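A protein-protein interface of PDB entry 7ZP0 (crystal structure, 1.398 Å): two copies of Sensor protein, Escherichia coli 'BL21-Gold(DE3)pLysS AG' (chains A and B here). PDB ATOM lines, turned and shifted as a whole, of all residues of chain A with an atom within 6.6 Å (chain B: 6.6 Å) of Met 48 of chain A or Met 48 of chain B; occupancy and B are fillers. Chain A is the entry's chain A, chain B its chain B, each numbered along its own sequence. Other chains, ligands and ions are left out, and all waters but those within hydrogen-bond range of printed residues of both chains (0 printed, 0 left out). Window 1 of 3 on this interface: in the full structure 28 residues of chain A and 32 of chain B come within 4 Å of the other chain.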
ATOM      1  N   ILE A  10      22.115 -14.679  25.741  1.00  0.00           N
ATOM      2  CA  ILE A  10      23.335 -15.476  25.777  1.00  0.00           C
ATOM      3  C   ILE A  10      24.141 -15.363  24.493  1.00  0.00           C
ATOM      4  O   ILE A  10      25.317 -15.720  24.471  1.00  0.00           O
ATOM      5  CB  ILE A  10      23.043 -16.961  26.028  1.00  0.00           C
ATOM      6  CG1 ILE A  10      22.336 -17.560  24.815  1.00  0.00           C
ATOM      7  CG2 ILE A  10      22.250 -17.143  27.314  1.00  0.00           C
ATOM      8  CD1 ILE A  10      21.987 -19.003  24.974  1.00  0.00           C
ATOM      9  N   PRO A  13      27.655 -12.888  24.659  1.00  0.00           N
ATOM     10  CA  PRO A  13      28.908 -13.440  25.200  1.00  0.00           C
ATOM     11  C   PRO A  13      29.507 -14.586  24.369  1.00  0.00           C
ATOM     12  O   PRO A  13      30.739 -14.669  24.254  1.00  0.00           O
ATOM     13  CB  PRO A  13      28.503 -13.938  26.596  1.00  0.00           C
ATOM     14  CG  PRO A  13      27.018 -14.040  26.574  1.00  0.00           C
ATOM     15  CD  PRO A  13      26.557 -12.972  25.640  1.00  0.00           C
ATOM     16  N   ILE A  14      28.661 -15.445  23.805  1.00  0.00           N
ATOM     17  CA  ILE A  14      29.116 -16.525  22.932  1.00  0.00           C
ATOM     18  C   ILE A  14      29.831 -15.946  21.721  1.00  0.00           C
ATOM     19  O   ILE A  14      30.943 -16.358  21.375  1.00  0.00           O
ATOM     20  CB  ILE A  14      27.942 -17.403  22.464  1.00  0.00           C
ATOM     21  CG1 ILE A  14      27.330 -18.119  23.663  1.00  0.00           C
ATOM     22  CG2 ILE A  14      28.422 -18.431  21.427  1.00  0.00           C
ATOM     23  CD1 ILE A  14      26.098 -18.934  23.325  1.00  0.00           C
ATOM     24  N   LEU A  17      33.239 -14.374  22.427  1.00  0.00           N
ATOM     25  CA  LEU A  17      34.283 -15.360  22.681  1.00  0.00           C
ATOM     26  C   LEU A  17      34.734 -16.019  21.396  1.00  0.00           C
ATOM     27  O   LEU A  17      35.923 -16.281  21.206  1.00  0.00           O
ATOM     28  CB  LEU A  17      33.805 -16.423  23.663  1.00  0.00           C
ATOM     29  CG  LEU A  17      34.023 -16.100  25.136  1.00  0.00           C
ATOM     30  CD1 LEU A  17      33.323 -17.126  26.007  1.00  0.00           C
ATOM     31  CD2 LEU A  17      35.510 -16.054  25.440  1.00  0.00           C
ATOM     32  N   ILE A  18      33.774 -16.305  20.523  1.00  0.00           N
ATOM     33  CA  ILE A  18      34.086 -16.884  19.228  1.00  0.00           C
ATOM     34  C   ILE A  18      34.960 -15.929  18.421  1.00  0.00           C
ATOM     35  O   ILE A  18      35.965 -16.342  17.836  1.00  0.00           O
ATOM     36  CB  ILE A  18      32.812 -17.222  18.437  1.00  0.00           C
ATOM     37  CG1 ILE A  18      32.121 -18.441  19.054  1.00  0.00           C
ATOM     38  CG2 ILE A  18      33.150 -17.477  16.978  1.00  0.00           C
ATOM     39  CD1 ILE A  18      30.853 -18.864  18.349  1.00  0.00           C
ATOM     40  N   GLU A  43      38.077 -15.477  31.948  1.00  0.00           N
ATOM     41  CA  GLU A  43      37.298 -14.449  32.625  1.00  0.00           C
ATOM     42  C   GLU A  43      35.879 -14.331  32.065  1.00  0.00           C
ATOM     43  O   GLU A  43      34.924 -14.123  32.818  1.00  0.00           O
ATOM     44  CB  GLU A  43      38.023 -13.106  32.527  1.00  0.00           C
ATOM     45  CG  GLU A  43      39.212 -12.993  33.470  1.00  0.00           C
ATOM     46  CD  GLU A  43      40.039 -11.752  33.215  1.00  0.00           C
ATOM     47  OE1 GLU A  43      39.868 -11.131  32.143  1.00  0.00           O
ATOM     48  OE2 GLU A  43      40.861 -11.394  34.084  1.00  0.00           O
ATOM     49  N   GLU A  44      35.739 -14.466  30.750  1.00  0.00           N
ATOM     50  CA  GLU A  44      34.432 -14.361  30.115  1.00  0.00           C
ATOM     51  C   GLU A  44      33.583 -15.602  30.395  1.00  0.00           C
ATOM     52  O   GLU A  44      32.391 -15.489  30.691  1.00  0.00           O
ATOM     53  CB  GLU A  44      34.580 -14.143  28.608  1.00  0.00           C
ATOM     54  CG  GLU A  44      33.263 -13.877  27.886  1.00  0.00           C
ATOM     55  CD  GLU A  44      32.492 -12.719  28.482  1.00  0.00           C
ATOM     56  OE1 GLU A  44      32.926 -11.564  28.296  1.00  0.00           O
ATOM     57  OE2 GLU A  44      31.451 -12.963  29.131  1.00  0.00           O
ATOM     58  N   LEU A  45      34.201 -16.779  30.307  1.00  0.00           N
ATOM     59  CA  LEU A  45      33.529 -18.032  30.648  1.00  0.00           C
ATOM     60  C   LEU A  45      33.048 -18.019  32.098  1.00  0.00           C
ATOM     61  O   LEU A  45      32.012 -18.600  32.422  1.00  0.00           O
ATOM     62  CB  LEU A  45      34.455 -19.237  30.424  1.00  0.00           C
ATOM     63  CG  LEU A  45      34.578 -19.905  29.042  1.00  0.00           C
ATOM     64  CD1 LEU A  45      33.210 -20.112  28.399  1.00  0.00           C
ATOM     65  CD2 LEU A  45      35.501 -19.153  28.095  1.00  0.00           C
ATOM     66  N   THR A  46      33.804 -17.354  32.966  1.00  0.00           N
ATOM     67  CA  THR A  46      33.421 -17.237  34.365  1.00  0.00           C
ATOM     68  C   THR A  46      32.149 -16.406  34.479  1.00  0.00           C
ATOM     69  O   THR A  46      31.265 -16.701  35.290  1.00  0.00           O
ATOM     70  CB  THR A  46      34.544 -16.604  35.208  1.00  0.00           C
ATOM     71  OG1 THR A  46      35.712 -17.430  35.144  1.00  0.00           O
ATOM     72  CG2 THR A  46      34.113 -16.462  36.661  1.00  0.00           C
ATOM     73  N   ARG A  47      32.051 -15.374  33.645  1.00  0.00           N
ATOM     74  CA  ARG A  47      30.873 -14.517  33.644  1.00  0.00           C
ATOM     75  C   ARG A  47      29.663 -15.258  33.089  1.00  0.00           C
ATOM     76  O   ARG A  47      28.555 -15.119  33.605  1.00  0.00           O
ATOM     77  CB  ARG A  47      31.134 -13.237  32.845  1.00  0.00           C
ATOM     78  CG  ARG A  47      32.194 -12.340  33.469  1.00  0.00           C
ATOM     79  CD  ARG A  47      32.271 -10.987  32.777  1.00  0.00           C
ATOM     80  NE  ARG A  47      33.498 -10.271  33.117  1.00  0.00           N
ATOM     81  CZ  ARG A  47      34.520 -10.097  32.283  1.00  0.00           C
ATOM     82  NH1 ARG A  47      34.463 -10.579  31.048  1.00  0.00           N
ATOM     83  NH2 ARG A  47      35.597  -9.432  32.680  1.00  0.00           N
ATOM     84  N   MET A  48      29.875 -16.053  32.043  1.00  0.00           N
ATOM     85  CA  MET A  48      28.795 -16.855  31.478  1.00  0.00           C
ATOM     86  C   MET A  48      28.295 -17.888  32.477  1.00  0.00           C
ATOM     87  O   MET A  48      27.109 -18.209  32.501  1.00  0.00           O
ATOM     88  CB  MET A  48      29.247 -17.558  30.196  1.00  0.00           C
ATOM     89  CG  MET A  48      29.759 -16.632  29.120  1.00  0.00           C
ATOM     90  SD  MET A  48      30.032 -17.550  27.597  1.00  0.00           S
ATOM     91  CE  MET A  48      28.386 -18.182  27.283  1.00  0.00           C
ATOM     92  N   ALA A  49      29.206 -18.408  33.295  1.00  0.00           N
ATOM     93  CA  ALA A  49      28.844 -19.362  34.341  1.00  0.00           C
ATOM     94  C   ALA A  49      27.990 -18.706  35.434  1.00  0.00           C
ATOM     95  O   ALA A  49      27.136 -19.359  36.034  1.00  0.00           O
ATOM     96  CB  ALA A  49      30.095 -19.989  34.945  1.00  0.00           C
ATOM     97  N   LYS A  50      28.224 -17.420  35.694  1.00  0.00           N
ATOM     98  CA  LYS A  50      27.380 -16.662  36.620  1.00  0.00           C
ATOM     99  C   LYS A  50      25.990 -16.474  36.020  1.00  0.00           C
ATOM    100  O   LYS A  50      24.978 -16.610  36.713  1.00  0.00           O
ATOM    101  CB  LYS A  50      28.014 -15.303  36.944  1.00  0.00           C
ATOM    102  CG  LYS A  50      27.189 -14.397  37.863  1.00  0.00           C
ATOM    103  CD  LYS A  50      26.760 -15.100  39.142  1.00  0.00           C
ATOM    104  CE  LYS A  50      26.195 -14.114  40.169  1.00  0.00           C
ATOM    105  NZ  LYS A  50      25.112 -13.257  39.615  1.00  0.00           N
ATOM    106  N   MET A  51      25.952 -16.146  34.734  1.00  0.00           N
ATOM    107  CA  MET A  51      24.707 -15.973  33.993  1.00  0.00           C
ATOM    108  C   MET A  51      23.802 -17.211  34.037  1.00  0.00           C
ATOM    109  O   MET A  51      22.606 -17.107  34.318  1.00  0.00           O
ATOM    110  CB  MET A  51      25.024 -15.612  32.542  1.00  0.00           C
ATOM    111  CG  MET A  51      23.836 -15.557  31.605  1.00  0.00           C
ATOM    112  SD  MET A  51      24.365 -15.140  29.926  1.00  0.00           S
ATOM    113  CE  MET A  51      25.489 -16.487  29.562  1.00  0.00           C
ATOM    114  N   VAL A  52      24.371 -18.382  33.757  1.00  0.00           N
ATOM    115  CA  VAL A  52      23.583 -19.608  33.706  1.00  0.00           C
ATOM    116  C   VAL A  52      23.063 -19.965  35.102  1.00  0.00           C
ATOM    117  O   VAL A  52      21.913 -20.387  35.256  1.00  0.00           O
ATOM    118  CB  VAL A  52      24.399 -20.794  33.103  1.00  0.00           C
ATOM    119  CG1 VAL A  52      25.672 -21.046  33.883  1.00  0.00           C
ATOM    120  CG2 VAL A  52      23.551 -22.058  33.042  1.00  0.00           C
ATOM    121  N   SER A  53      23.898 -19.767  36.116  1.00  0.00           N
ATOM    122  CA  SER A  53      23.505 -20.042  37.492  1.00  0.00           C
ATOM    123  C   SER A  53      22.370 -19.118  37.924  1.00  0.00           C
ATOM    124  O   SER A  53      21.483 -19.522  38.674  1.00  0.00           O
ATOM    125  CB  SER A  53      24.696 -19.894  38.435  1.00  0.00           C
ATOM    126  OG  SER A  53      25.332 -18.648  38.247  1.00  0.00           O
ATOM    127  N   ILE B  10      23.389 -25.540  28.488  1.00  0.00           N
ATOM    128  CA  ILE B  10      24.622 -24.775  28.358  1.00  0.00           C
ATOM    129  C   ILE B  10      25.549 -24.929  29.570  1.00  0.00           C
ATOM    130  O   ILE B  10      26.760 -24.737  29.461  1.00  0.00           O
ATOM    131  CB  ILE B  10      24.296 -23.293  28.134  1.00  0.00           C
ATOM    132  CG1 ILE B  10      23.328 -23.160  26.960  1.00  0.00           C
ATOM    133  CG2 ILE B  10      25.544 -22.497  27.849  1.00  0.00           C
ATOM    134  CD1 ILE B  10      22.770 -21.788  26.809  1.00  0.00           C
ATOM    135  N   PRO B  13      28.567 -27.500  28.727  1.00  0.00           N
ATOM    136  CA  PRO B  13      29.636 -26.982  27.860  1.00  0.00           C
ATOM    137  C   PRO B  13      30.428 -25.824  28.472  1.00  0.00           C
ATOM    138  O   PRO B  13      31.645 -25.761  28.277  1.00  0.00           O
ATOM    139  CB  PRO B  13      28.886 -26.518  26.598  1.00  0.00           C
ATOM    140  CG  PRO B  13      27.446 -26.582  26.925  1.00  0.00           C
ATOM    141  CD  PRO B  13      27.301 -27.618  27.990  1.00  0.00           C
ATOM    142  N   ILE B  14      29.760 -24.929  29.194  1.00  0.00           N
ATOM    143  CA  ILE B  14      30.457 -23.858  29.897  1.00  0.00           C
ATOM    144  C   ILE B  14      31.455 -24.440  30.893  1.00  0.00           C
ATOM    145  O   ILE B  14      32.618 -24.037  30.933  1.00  0.00           O
ATOM    146  CB  ILE B  14      29.480 -22.935  30.642  1.00  0.00           C
ATOM    147  CG1 ILE B  14      28.594 -22.191  29.648  1.00  0.00           C
ATOM    148  CG2 ILE B  14      30.240 -21.936  31.494  1.00  0.00           C
ATOM    149  CD1 ILE B  14      29.359 -21.373  28.654  1.00  0.00           C
ATOM    150  N   LEU B  17      34.560 -25.881  29.270  1.00  0.00           N
ATOM    151  CA  LEU B  17      35.458 -24.858  28.744  1.00  0.00           C
ATOM    152  C   LEU B  17      36.325 -24.261  29.844  1.00  0.00           C
ATOM    153  O   LEU B  17      37.529 -24.084  29.664  1.00  0.00           O
ATOM    154  CB  LEU B  17      34.668 -23.754  28.039  1.00  0.00           C
ATOM    155  CG  LEU B  17      34.210 -24.098  26.620  1.00  0.00           C
ATOM    156  CD1 LEU B  17      34.077 -22.836  25.793  1.00  0.00           C
ATOM    157  CD2 LEU B  17      35.176 -25.070  25.959  1.00  0.00           C
ATOM    158  N   GLU B  43      35.306 -25.176  18.972  1.00  0.00           N
ATOM    159  CA  GLU B  43      34.375 -26.231  18.581  1.00  0.00           C
ATOM    160  C   GLU B  43      33.138 -26.227  19.474  1.00  0.00           C
ATOM    161  O   GLU B  43      32.014 -26.353  18.991  1.00  0.00           O
ATOM    162  CB  GLU B  43      35.059 -27.598  18.635  1.00  0.00           C
ATOM    163  CG  GLU B  43      36.153 -27.790  17.600  1.00  0.00           C
ATOM    164  CD  GLU B  43      37.158 -28.856  18.001  1.00  0.00           C
ATOM    165  OE1 GLU B  43      36.952 -29.510  19.045  1.00  0.00           O
ATOM    166  OE2 GLU B  43      38.160 -29.034  17.275  1.00  0.00           O
ATOM    167  N   GLU B  44      33.356 -26.082  20.779  1.00  0.00           N
ATOM    168  CA  GLU B  44      32.269 -26.051  21.746  1.00  0.00           C
ATOM    169  C   GLU B  44      31.455 -24.774  21.598  1.00  0.00           C
ATOM    170  O   GLU B  44      30.222 -24.803  21.627  1.00  0.00           O
ATOM    171  CB  GLU B  44      32.808 -26.163  23.173  1.00  0.00           C
ATOM    172  CG  GLU B  44      33.564 -27.445  23.466  1.00  0.00           C
ATOM    173  CD  GLU B  44      32.909 -28.271  24.559  1.00  0.00           C
ATOM    174  OE1 GLU B  44      33.558 -29.212  25.063  1.00  0.00           O
ATOM    175  OE2 GLU B  44      31.745 -27.982  24.910  1.00  0.00           O
ATOM    176  N   LEU B  45      32.154 -23.651  21.450  1.00  0.00           N
ATOM    177  CA  LEU B  45      31.496 -22.356  21.281  1.00  0.00           C
ATOM    178  C   LEU B  45      30.669 -22.335  20.001  1.00  0.00           C
ATOM    179  O   LEU B  45      29.601 -21.723  19.950  1.00  0.00           O
ATOM    180  CB  LEU B  45      32.523 -21.221  21.262  1.00  0.00           C
ATOM    181  CG  LEU B  45      33.300 -20.912  22.546  1.00  0.00           C
ATOM    182  CD1 LEU B  45      34.391 -19.899  22.271  1.00  0.00           C
ATOM    183  CD2 LEU B  45      32.365 -20.399  23.627  1.00  0.00           C
ATOM    184  N   THR B  46      31.169 -23.013  18.972  1.00  0.00           N
ATOM    185  CA  THR B  46      30.470 -23.103  17.695  1.00  0.00           C
ATOM    186  C   THR B  46      29.161 -23.870  17.830  1.00  0.00           C
ATOM    187  O   THR B  46      28.164 -23.505  17.222  1.00  0.00           O
ATOM    188  CB  THR B  46      31.345 -23.778  16.624  1.00  0.00           C
ATOM    189  OG1 THR B  46      32.567 -23.052  16.492  1.00  0.00           O
ATOM    190  CG2 THR B  46      30.633 -23.797  15.280  1.00  0.00           C
ATOM    191  N   ARG B  47      29.168 -24.937  18.622  1.00  0.00           N
ATOM    192  CA  ARG B  47      27.940 -25.682  18.879  1.00  0.00           C
ATOM    193  C   ARG B  47      26.942 -24.822  19.641  1.00  0.00           C
ATOM    194  O   ARG B  47      25.734 -24.903  19.409  1.00  0.00           O
ATOM    195  CB  ARG B  47      28.223 -26.963  19.666  1.00  0.00           C
ATOM    196  CG  ARG B  47      29.183 -27.918  18.984  1.00  0.00           C
ATOM    197  CD  ARG B  47      29.113 -29.300  19.607  1.00  0.00           C
ATOM    198  NE  ARG B  47      30.423 -29.757  20.059  1.00  0.00           N
ATOM    199  CZ  ARG B  47      30.796 -29.797  21.333  1.00  0.00           C
ATOM    200  NH1 ARG B  47      29.951 -29.416  22.282  1.00  0.00           N
ATOM    201  NH2 ARG B  47      32.008 -30.221  21.661  1.00  0.00           N
ATOM    202  N   MET B  48      27.443 -23.997  20.554  1.00  0.00           N
ATOM    203  CA  MET B  48      26.574 -23.124  21.329  1.00  0.00           C
ATOM    204  C   MET B  48      25.905 -22.106  20.420  1.00  0.00           C
ATOM    205  O   MET B  48      24.706 -21.836  20.554  1.00  0.00           O
ATOM    206  CB  MET B  48      27.366 -22.429  22.438  1.00  0.00           C
ATOM    207  CG  MET B  48      27.805 -23.388  23.540  1.00  0.00           C
ATOM    208  SD  MET B  48      28.829 -22.622  24.805  1.00  0.00           S
ATOM    209  CE  MET B  48      27.759 -21.314  25.368  1.00  0.00           C
ATOM    210  N   ALA B  49      26.670 -21.563  19.476  1.00  0.00           N
ATOM    211  CA  ALA B  49      26.133 -20.556  18.562  1.00  0.00           C
ATOM    212  C   ALA B  49      25.068 -21.159  17.654  1.00  0.00           C
ATOM    213  O   ALA B  49      24.079 -20.489  17.328  1.00  0.00           O
ATOM    214  CB  ALA B  49      27.244 -19.931  17.746  1.00  0.00           C
ATOM    215  N   LYS B  50      25.270 -22.418  17.264  1.00  0.00           N
ATOM    216  CA  LYS B  50      24.283 -23.160  16.492  1.00  0.00           C
ATOM    217  C   LYS B  50      22.996 -23.349  17.294  1.00  0.00           C
ATOM    218  O   LYS B  50      21.888 -23.231  16.757  1.00  0.00           O
ATOM    219  CB  LYS B  50      24.853 -24.511  16.071  1.00  0.00           C
ATOM    220  CG  LYS B  50      23.805 -25.512  15.631  1.00  0.00           C
ATOM    221  CD  LYS B  50      23.186 -25.113  14.310  1.00  0.00           C
ATOM    222  CE  LYS B  50      22.261 -26.216  13.811  1.00  0.00           C
ATOM    223  NZ  LYS B  50      21.477 -25.843  12.615  1.00  0.00           N
ATOM    224  N   MET B  51      23.143 -23.664  18.577  1.00  0.00           N
ATOM    225  CA  MET B  51      21.981 -23.805  19.450  1.00  0.00           C
ATOM    226  C   MET B  51      21.201 -22.495  19.505  1.00  0.00           C
ATOM    227  O   MET B  51      19.974 -22.491  19.447  1.00  0.00           O
ATOM    228  CB  MET B  51      22.393 -24.230  20.863  1.00  0.00           C
ATOM    229  CG  MET B  51      21.220 -24.318  21.840  1.00  0.00           C
ATOM    230  SD  MET B  51      21.676 -24.327  23.588  1.00  0.00           S
ATOM    231  CE  MET B  51      20.081 -24.057  24.354  1.00  0.00           C
ATOM    232  N   VAL B  52      21.921 -21.383  19.614  1.00  0.00           N
ATOM    233  CA  VAL B  52      21.284 -20.069  19.665  1.00  0.00           C
ATOM    234  C   VAL B  52      20.532 -19.778  18.370  1.00  0.00           C
ATOM    235  O   VAL B  52      19.378 -19.350  18.396  1.00  0.00           O
ATOM    236  CB  VAL B  52      22.316 -18.952  19.937  1.00  0.00           C
ATOM    237  CG1 VAL B  52      21.741 -17.597  19.595  1.00  0.00           C
ATOM    238  CG2 VAL B  52      22.780 -19.006  21.383  1.00  0.00           C
ATOM    239  N   SER B  53      21.181 -20.035  17.240  1.00  0.00           N
ATOM    240  CA  SER B  53      20.557 -19.861  15.931  1.00  0.00           C
ATOM    241  C   SER B  53      19.287 -20.695  15.783  1.00  0.00           C
ATOM    242  O   SER B  53      18.262 -20.207  15.293  1.00  0.00           O
ATOM    243  CB  SER B  53      21.537 -20.236  14.826  1.00  0.00           C
ATOM    244  OG  SER B  53      20.952 -20.080  13.547  1.00  0.00           O
ATOM    245  N   MET B  55      17.367 -21.766  18.192  1.00  0.00           N
ATOM    246  CA  MET B  55      16.324 -21.248  19.084  1.00  0.00           C
ATOM    247  C   MET B  55      15.587 -20.053  18.493  1.00  0.00           C
ATOM    248  O   MET B  55      14.359 -19.948  18.642  1.00  0.00           O
ATOM    249  CB  MET B  55      16.906 -20.878  20.447  1.00  0.00           C
ATOM    250  CG  MET B  55      17.272 -22.103  21.262  1.00  0.00           C
ATOM    251  SD  MET B  55      17.695 -21.704  22.957  1.00  0.00           S
ATOM    252  CE  MET B  55      19.179 -20.757  22.677  1.00  0.00           C
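Ile 10 of chain B touches its own counterpart, Ile 10 of chain A. Ile 14 of chain A touches Val 52 of chain B, but with the chains exchanged Val 52 of chain A does not touch Ile 14 of chain B (5.2 Å). Leu 17 of chain A touches Leu 45 of chain B, and with the chains exchanged Leu 45 of chain A touches Leu 17 of chain B. Met 48 of chain B touches its own counterpart, Met 48 of chain A. Positions printed for both chains: 10, 13, 14, 17, 43, 44, 45, 46, 47, 48, 49, 50, 51, 52 and 53. Of the 13 pairs that touch across the chains among the printed residues, 8 have their exchanged pair printed and touching as well.
OG of Ser 53 of chain A lies within hydrogen-bond range of O of Ala 49 of chain A (2.9 Å).
Among the printed residues, pairs that only touch across the chains: Ile 10 of chain A with Ile 10 of chain B (3.4 Å), Ile 18 of chain A with Leu 45 of chain B (3.5 Å), Ile 14 of chain A with Met 48 of chain B (3.5 Å), Met 48 of chain A with Ile 14 of chain B (3.6 Å), Ile 10 of chain A with Val 52 of chain B (3.7 Å), Met 48 of chain A with Met 48 of chain B (3.7 Å), Leu 17 of chain A with Leu 45 of chain B (3.8 Å), Ile 14 of chain A with Leu 45 of chain B (3.8 Å), Ile 18 of chain A with Ala 49 of chain B (3.8 Å), Ile 14 of chain A with Val 52 of chain B (3.8 Å), Leu 45 of chain A with Leu 17 of chain B (3.9 Å), Leu 45 of chain A with Ile 14 of chain B (3.9 Å) and Ala 49 of chain A with Ile 14 of chain B (3.97 Å).
Printed residues of chain B within 4 Å of Ile 10 of chain A: Ile 10 and Val 52. Printed residues of chain B within 4 Å of Ile 14 of chain A: Leu 45, Met 48 and Val 52. Met 48 of chain A touches just these residues of chain B: Ile 14 and Met 48. Of the printed residues of chain A, Ile 10 of chain B touches Ile 10. Of the printed residues of chain A, Ile 14 of chain B touches Leu 45, Met 48 and Ala 49. Glu 44 of chain B touches none of the printed residues of chain A. Arg 47 of chain B touches none of the printed residues of chain A. Of chain A, only Ile 14 (3.5 Å) and Met 48 (3.7 Å) come within 4 Å of Met 48 of chain B. Of the printed residues of chain A, Val 52 of chain B touches Ile 10 and Ile 14. The nearest residue of chain B that does not touch Met 48 of chain A is Ile 10 of chain B (5.2 Å). The nearest residue of chain A that does not touch Met 48 of chain B is Ile 10 of chain A (5.9 Å).
Of the 16 printed residues of chain A, 7 touch a printed residue of chain B. Hydrophobic or aromatic side chains of chain B within 4 Å of the printed part of chain A: Ile 10, Ile 14, Leu 17, Leu 45, Met 48, Ala 49 and Val 52.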
